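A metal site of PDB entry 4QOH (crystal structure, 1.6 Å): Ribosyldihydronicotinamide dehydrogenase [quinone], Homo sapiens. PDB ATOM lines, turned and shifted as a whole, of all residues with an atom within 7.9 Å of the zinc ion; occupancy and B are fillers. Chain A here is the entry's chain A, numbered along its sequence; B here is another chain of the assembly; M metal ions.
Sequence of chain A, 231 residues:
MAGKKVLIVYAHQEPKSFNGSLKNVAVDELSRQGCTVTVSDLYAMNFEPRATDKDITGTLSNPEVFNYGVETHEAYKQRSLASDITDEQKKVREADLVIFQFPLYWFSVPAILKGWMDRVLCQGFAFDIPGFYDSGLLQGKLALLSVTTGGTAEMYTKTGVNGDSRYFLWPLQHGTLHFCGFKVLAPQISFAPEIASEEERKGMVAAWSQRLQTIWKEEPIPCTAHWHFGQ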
ATOM      1  N   TYR A 133     -17.945  21.517 -16.415  1.00  0.00           N
ATOM      2  CA  TYR A 133     -16.920  21.489 -17.417  1.00  0.00           C
ATOM      3  C   TYR A 133     -16.121  20.188 -17.262  1.00  0.00           C
ATOM      4  O   TYR A 133     -16.692  19.130 -17.229  1.00  0.00           O
ATOM      5  CB  TYR A 133     -16.093  22.792 -17.430  1.00  0.00           C
ATOM      6  CG  TYR A 133     -16.826  23.953 -18.084  1.00  0.00           C
ATOM      7  CD1 TYR A 133     -17.284  23.859 -19.378  1.00  0.00           C
ATOM      8  CD2 TYR A 133     -17.057  25.148 -17.417  1.00  0.00           C
ATOM      9  CE1 TYR A 133     -17.959  24.883 -19.960  1.00  0.00           C
ATOM     10  CE2 TYR A 133     -17.720  26.191 -18.029  1.00  0.00           C
ATOM     11  CZ  TYR A 133     -18.182  26.037 -19.293  1.00  0.00           C
ATOM     12  OH  TYR A 133     -18.880  27.034 -19.916  1.00  0.00           O
ATOM     13  N   ASP A 134     -14.805  20.271 -17.133  1.00  0.00           N
ATOM     14  CA  ASP A 134     -14.006  19.049 -16.998  1.00  0.00           C
ATOM     15  C   ASP A 134     -14.459  18.172 -15.838  1.00  0.00           C
ATOM     16  O   ASP A 134     -14.259  17.006 -15.865  1.00  0.00           O
ATOM     17  CB  ASP A 134     -12.517  19.342 -16.936  1.00  0.00           C
ATOM     18  CG  ASP A 134     -11.949  19.796 -18.253  1.00  0.00           C
ATOM     19  OD1 ASP A 134     -12.653  19.833 -19.234  1.00  0.00           O
ATOM     20  OD2 ASP A 134     -10.761  20.119 -18.294  1.00  0.00           O
ATOM     21  N   TRP A 170     -20.648  26.713 -30.598  1.00  0.00           N
ATOM     22  CA  TRP A 170     -20.173  27.081 -29.260  1.00  0.00           C
ATOM     23  C   TRP A 170     -21.194  26.771 -28.147  1.00  0.00           C
ATOM     24  O   TRP A 170     -20.878  26.122 -27.137  1.00  0.00           O
ATOM     25  CB  TRP A 170     -19.698  28.605 -29.242  1.00  0.00           C
ATOM     26  CG  TRP A 170     -19.315  29.184 -27.887  1.00  0.00           C
ATOM     27  CD1 TRP A 170     -19.989  30.129 -27.220  1.00  0.00           C
ATOM     28  CD2 TRP A 170     -18.120  28.921 -27.135  1.00  0.00           C
ATOM     29  NE1 TRP A 170     -19.353  30.430 -26.030  1.00  0.00           N
ATOM     30  CE2 TRP A 170     -18.176  29.714 -25.987  1.00  0.00           C
ATOM     31  CE3 TRP A 170     -17.011  28.099 -27.341  1.00  0.00           C
ATOM     32  CZ2 TRP A 170     -17.185  29.664 -24.998  1.00  0.00           C
ATOM     33  CZ3 TRP A 170     -16.039  28.068 -26.390  1.00  0.00           C
ATOM     34  CH2 TRP A 170     -16.147  28.824 -25.211  1.00  0.00           C
ATOM     35  N   LEU A 172     -23.674  24.729 -28.053  1.00  0.00           N
ATOM     36  CA  LEU A 172     -23.933  23.298 -28.013  1.00  0.00           C
ATOM     37  C   LEU A 172     -22.726  22.507 -27.444  1.00  0.00           C
ATOM     38  O   LEU A 172     -22.871  21.761 -26.485  1.00  0.00           O
ATOM     39  CB  LEU A 172     -24.352  22.838 -29.395  1.00  0.00           C
ATOM     40  CG  LEU A 172     -25.564  23.552 -29.886  1.00  0.00           C
ATOM     41  CD1 LEU A 172     -25.655  23.173 -31.349  1.00  0.00           C
ATOM     42  CD2 LEU A 172     -26.837  23.131 -29.254  1.00  0.00           C
ATOM     43  N   GLN A 173     -21.548  22.702 -28.060  1.00  0.00           N
ATOM     44  CA  GLN A 173     -20.282  21.980 -27.677  1.00  0.00           C
ATOM     45  C   GLN A 173     -19.751  22.425 -26.331  1.00  0.00           C
ATOM     46  O   GLN A 173     -19.604  21.591 -25.440  1.00  0.00           O
ATOM     47  CB  GLN A 173     -19.251  22.128 -28.757  1.00  0.00           C
ATOM     48  CG  GLN A 173     -19.780  21.483 -30.073  1.00  0.00           C
ATOM     49  CD  GLN A 173     -18.698  21.236 -31.050  1.00  0.00           C
ATOM     50  OE1 GLN A 173     -18.752  20.286 -31.827  1.00  0.00           O
ATOM     51  NE2 GLN A 173     -17.675  22.084 -31.043  1.00  0.00           N
ATOM     52  N   HIS A 174     -19.624  23.766 -26.178  1.00  0.00           N
ATOM     53  CA  HIS A 174     -19.042  24.292 -24.958  1.00  0.00           C
ATOM     54  C   HIS A 174     -20.086  24.521 -23.886  1.00  0.00           C
ATOM     55  O   HIS A 174     -20.024  23.929 -22.768  1.00  0.00           O
ATOM     56  CB  HIS A 174     -18.227  25.538 -25.255  1.00  0.00           C
ATOM     57  CG  HIS A 174     -17.559  26.076 -24.026  1.00  0.00           C
ATOM     58  ND1 HIS A 174     -16.304  25.681 -23.669  1.00  0.00           N
ATOM     59  CD2 HIS A 174     -17.961  26.958 -23.077  1.00  0.00           C
ATOM     60  CE1 HIS A 174     -15.964  26.246 -22.528  1.00  0.00           C
ATOM     61  NE2 HIS A 174     -16.931  27.052 -22.157  1.00  0.00           N
ATOM     62  N   GLY A 175     -21.090  25.329 -24.179  1.00  0.00           N
ATOM     63  CA  GLY A 175     -22.027  25.718 -23.157  1.00  0.00           C
ATOM     64  C   GLY A 175     -22.883  24.645 -22.548  1.00  0.00           C
ATOM     65  O   GLY A 175     -23.313  24.766 -21.441  1.00  0.00           O
ATOM     66  N   THR A 176     -23.118  23.597 -23.310  1.00  0.00           N
ATOM     67  CA  THR A 176     -23.932  22.481 -22.924  1.00  0.00           C
ATOM     68  C   THR A 176     -23.129  21.211 -22.649  1.00  0.00           C
ATOM     69  O   THR A 176     -23.008  20.755 -21.553  1.00  0.00           O
ATOM     70  CB  THR A 176     -24.963  22.203 -24.041  1.00  0.00           C
ATOM     71  OG1 THR A 176     -25.627  23.392 -24.336  1.00  0.00           O
ATOM     72  CG2 THR A 176     -25.962  21.186 -23.565  1.00  0.00           C
ATOM     73  N   LEU A 177     -22.556  20.673 -23.689  1.00  0.00           N
ATOM     74  CA  LEU A 177     -21.941  19.376 -23.652  1.00  0.00           C
ATOM     75  C   LEU A 177     -20.657  19.368 -22.814  1.00  0.00           C
ATOM     76  O   LEU A 177     -20.523  18.599 -21.956  1.00  0.00           O
ATOM     77  CB  LEU A 177     -21.647  18.889 -25.061  1.00  0.00           C
ATOM     78  CG  LEU A 177     -22.907  18.677 -25.891  1.00  0.00           C
ATOM     79  CD1 LEU A 177     -22.548  18.280 -27.285  1.00  0.00           C
ATOM     80  CD2 LEU A 177     -23.805  17.638 -25.262  1.00  0.00           C
ATOM     81  N   HIS A 178     -19.765  20.279 -23.130  1.00  0.00           N
ATOM     82  CA  HIS A 178     -18.486  20.410 -22.292  1.00  0.00           C
ATOM     83  C   HIS A 178     -18.875  20.763 -20.899  1.00  0.00           C
ATOM     84  O   HIS A 178     -18.326  20.166 -19.962  1.00  0.00           O
ATOM     85  CB  HIS A 178     -17.557  21.403 -22.886  1.00  0.00           C
ATOM     86  CG  HIS A 178     -16.217  21.494 -22.213  1.00  0.00           C
ATOM     87  ND1 HIS A 178     -15.320  22.473 -22.550  1.00  0.00           N
ATOM     88  CD2 HIS A 178     -15.651  20.816 -21.185  1.00  0.00           C
ATOM     89  CE1 HIS A 178     -14.237  22.361 -21.798  1.00  0.00           C
ATOM     90  NE2 HIS A 178     -14.424  21.373 -20.964  1.00  0.00           N
ATOM     91  N   PHE A 179     -19.875  21.651 -20.689  1.00  0.00           N
ATOM     92  CA  PHE A 179     -20.317  21.964 -19.333  1.00  0.00           C
ATOM     93  C   PHE A 179     -20.612  20.721 -18.552  1.00  0.00           C
ATOM     94  O   PHE A 179     -20.282  20.652 -17.333  1.00  0.00           O
ATOM     95  CB  PHE A 179     -21.460  23.022 -19.291  1.00  0.00           C
ATOM     96  CG  PHE A 179     -21.831  23.493 -17.919  1.00  0.00           C
ATOM     97  CD1 PHE A 179     -21.198  24.588 -17.341  1.00  0.00           C
ATOM     98  CD2 PHE A 179     -22.814  22.915 -17.245  1.00  0.00           C
ATOM     99  CE1 PHE A 179     -21.599  25.029 -16.088  1.00  0.00           C
ATOM    100  CE2 PHE A 179     -23.246  23.313 -16.017  1.00  0.00           C
ATOM    101  CZ  PHE A 179     -22.603  24.398 -15.408  1.00  0.00           C
ATOM    102  N   PHE A 182     -18.844  16.087 -20.959  1.00  0.00           N
ATOM    103  CA  PHE A 182     -18.567  15.355 -22.129  1.00  0.00           C
ATOM    104  C   PHE A 182     -17.259  15.760 -22.778  1.00  0.00           C
ATOM    105  O   PHE A 182     -16.873  16.948 -22.805  1.00  0.00           O
ATOM    106  CB  PHE A 182     -19.649  15.547 -23.242  1.00  0.00           C
ATOM    107  CG  PHE A 182     -20.952  14.826 -23.020  1.00  0.00           C
ATOM    108  CD1 PHE A 182     -21.101  13.510 -23.449  1.00  0.00           C
ATOM    109  CD2 PHE A 182     -22.069  15.522 -22.524  1.00  0.00           C
ATOM    110  CE1 PHE A 182     -22.339  12.883 -23.316  1.00  0.00           C
ATOM    111  CE2 PHE A 182     -23.292  14.927 -22.425  1.00  0.00           C
ATOM    112  CZ  PHE A 182     -23.412  13.604 -22.789  1.00  0.00           C
ATOM    113  N   VAL A 184     -15.956  16.057 -26.432  1.00  0.00           N
ATOM    114  CA  VAL A 184     -16.648  16.302 -27.736  1.00  0.00           C
ATOM    115  C   VAL A 184     -15.838  15.848 -28.923  1.00  0.00           C
ATOM    116  O   VAL A 184     -14.745  16.336 -29.204  1.00  0.00           O
ATOM    117  CB  VAL A 184     -17.057  17.796 -27.880  1.00  0.00           C
ATOM    118  CG1 VAL A 184     -17.752  18.068 -29.231  1.00  0.00           C
ATOM    119  CG2 VAL A 184     -17.787  18.247 -26.667  1.00  0.00           C
ATOM    120  N   ILE A 221     -12.058  16.926 -29.551  1.00  0.00           N
ATOM    121  CA  ILE A 221     -11.478  18.244 -29.718  1.00  0.00           C
ATOM    122  C   ILE A 221     -11.095  18.892 -28.392  1.00  0.00           C
ATOM    123  O   ILE A 221     -11.607  18.557 -27.311  1.00  0.00           O
ATOM    124  CB  ILE A 221     -12.441  19.187 -30.432  1.00  0.00           C
ATOM    125  CG1 ILE A 221     -13.721  19.457 -29.602  1.00  0.00           C
ATOM    126  CG2 ILE A 221     -12.755  18.672 -31.808  1.00  0.00           C
ATOM    127  CD1 ILE A 221     -14.551  20.562 -30.211  1.00  0.00           C
ATOM    128  N   PRO A 222     -10.229  19.926 -28.479  1.00  0.00           N
ATOM    129  CA  PRO A 222     -10.111  20.745 -27.313  1.00  0.00           C
ATOM    130  C   PRO A 222     -11.266  21.751 -27.419  1.00  0.00           C
ATOM    131  O   PRO A 222     -11.239  22.599 -28.279  1.00  0.00           O
ATOM    132  CB  PRO A 222      -8.766  21.436 -27.509  1.00  0.00           C
ATOM    133  CG  PRO A 222      -8.587  21.500 -29.000  1.00  0.00           C
ATOM    134  CD  PRO A 222      -9.586  20.534 -29.646  1.00  0.00           C
ATOM    135  N   CYS A 223     -12.208  21.649 -26.494  1.00  0.00           N
ATOM    136  CA  CYS A 223     -13.483  22.411 -26.535  1.00  0.00           C
ATOM    137  C   CYS A 223     -13.258  23.729 -25.782  1.00  0.00           C
ATOM    138  O   CYS A 223     -13.553  23.891 -24.558  1.00  0.00           O
ATOM    139  CB  CYS A 223     -14.652  21.598 -25.988  1.00  0.00           C
ATOM    140  SG  CYS A 223     -16.203  22.572 -26.026  1.00  0.00           S
ATOM    141  N   THR A 224     -12.562  24.586 -26.500  1.00  0.00           N
ATOM    142  CA  THR A 224     -12.130  25.879 -25.993  1.00  0.00           C
ATOM    143  C   THR A 224     -12.531  26.983 -26.922  1.00  0.00           C
ATOM    144  O   THR A 224     -12.795  26.813 -28.097  1.00  0.00           O
ATOM    145  CB  THR A 224     -10.565  25.920 -25.925  1.00  0.00           C
ATOM    146  OG1 THR A 224     -10.052  25.797 -27.258  1.00  0.00           O
ATOM    147  CG2 THR A 224      -9.983  24.871 -25.007  1.00  0.00           C
ATOM    148  N   ALA A 225     -12.492  28.221 -26.404  1.00  0.00           N
ATOM    149  CA  ALA A 225     -12.694  29.400 -27.186  1.00  0.00           C
ATOM    150  C   ALA A 225     -11.799  29.439 -28.375  1.00  0.00           C
ATOM    151  O   ALA A 225     -12.216  29.651 -29.539  1.00  0.00           O
ATOM    152  CB  ALA A 225     -12.466  30.638 -26.301  1.00  0.00           C
ATOM    153  N   TRP A 227     -10.430  26.982 -30.166  1.00  0.00           N
ATOM    154  CA  TRP A 227     -10.820  26.056 -31.199  1.00  0.00           C
ATOM    155  C   TRP A 227     -12.011  26.632 -32.006  1.00  0.00           C
ATOM    156  O   TRP A 227     -12.039  26.602 -33.264  1.00  0.00           O
ATOM    157  CB  TRP A 227     -11.224  24.728 -30.545  1.00  0.00           C
ATOM    158  CG  TRP A 227     -11.526  23.699 -31.513  1.00  0.00           C
ATOM    159  CD1 TRP A 227     -10.647  22.761 -31.994  1.00  0.00           C
ATOM    160  CD2 TRP A 227     -12.788  23.433 -32.176  1.00  0.00           C
ATOM    161  NE1 TRP A 227     -11.270  21.980 -32.961  1.00  0.00           N
ATOM    162  CE2 TRP A 227     -12.593  22.335 -33.039  1.00  0.00           C
ATOM    163  CE3 TRP A 227     -14.075  23.989 -32.088  1.00  0.00           C
ATOM    164  CZ2 TRP A 227     -13.621  21.777 -33.823  1.00  0.00           C
ATOM    165  CZ3 TRP A 227     -15.092  23.451 -32.902  1.00  0.00           C
ATOM    166  CH2 TRP A 227     -14.859  22.367 -33.752  1.00  0.00           C
ATOM    167  N   HIS A 228     -12.972  27.201 -31.285  1.00  0.00           N
ATOM    168  CA  HIS A 228     -14.187  27.726 -31.938  1.00  0.00           C
ATOM    169  C   HIS A 228     -13.938  29.070 -32.715  1.00  0.00           C
ATOM    170  O   HIS A 228     -14.406  29.299 -33.842  1.00  0.00           O
ATOM    171  CB  HIS A 228     -15.293  27.859 -30.903  1.00  0.00           C
ATOM    172  CG  HIS A 228     -15.804  26.551 -30.330  1.00  0.00           C
ATOM    173  ND1 HIS A 228     -15.290  25.968 -29.182  1.00  0.00           N
ATOM    174  CD2 HIS A 228     -16.861  25.788 -30.691  1.00  0.00           C
ATOM    175  CE1 HIS A 228     -15.976  24.876 -28.902  1.00  0.00           C
ATOM    176  NE2 HIS A 228     -16.970  24.768 -29.770  1.00  0.00           N
ATOM    177  N   VAL B 161     -14.385  31.124 -17.840  1.00  0.00           N
ATOM    178  CA  VAL B 161     -14.786  29.721 -18.148  1.00  0.00           C
ATOM    179  C   VAL B 161     -15.903  29.689 -19.163  1.00  0.00           C
ATOM    180  O   VAL B 161     -16.045  28.686 -19.900  1.00  0.00           O
ATOM    181  CB  VAL B 161     -15.285  28.920 -16.959  1.00  0.00           C
ATOM    182  CG1 VAL B 161     -14.174  28.571 -15.972  1.00  0.00           C
ATOM    183  CG2 VAL B 161     -16.504  29.521 -16.308  1.00  0.00           C
HETATM  184 ZN    ZN M   1     -15.641  23.617 -24.232  1.00  0.00          ZN
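N of His 178 lies within hydrogen-bond range of O of Gln 173 (2.7 Å).
OD1 of Asp 134 is in hydrogen-bond range of NE2 of His 178 (2.9 Å).
The side-chain sulfur of Cys 223 lies close to the backbone carbonyl oxygen of Gln 173.
A ring nitrogen (NE2) of His 174 is in hydrogen-bond range of the side-chain hydroxyl (OH) of Tyr 133 (3.0 Å).
The backbone NH of Phe 179 lies within hydrogen-bond range of the backbone carbonyl oxygen of His 174 (3.1 Å).
A ring nitrogen (NE2) of His 174 sits at hydrogen-bond distance from the backbone carbonyl oxygen of Val 161 of chain B (2.9 Å).
O of Thr 224 lies within hydrogen-bond range of ND1 of His 228.
The backbone NH of Trp 227 lies within hydrogen-bond range of the side-chain hydroxyl of Thr 224 (3.2 Å).
Residues that only touch the zinc ion: Thr 224 (3.9 Å).
Four residues have an atom within 4 Å of the zinc ion: His 174, His 178, Cys 223 and Thr 224.
The zinc ion is bound by a ring nitrogen (ND1) of His 178 (2.1 Å), the backbone carbonyl oxygen (O) of Cys 223 (2.1 Å), the side-chain sulfur (SG) of Cys 223 (2.2 Å) and a ring nitrogen (ND1) of His 174 (2.2 Å).
The zinc ion has four donor atoms within binding distance.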
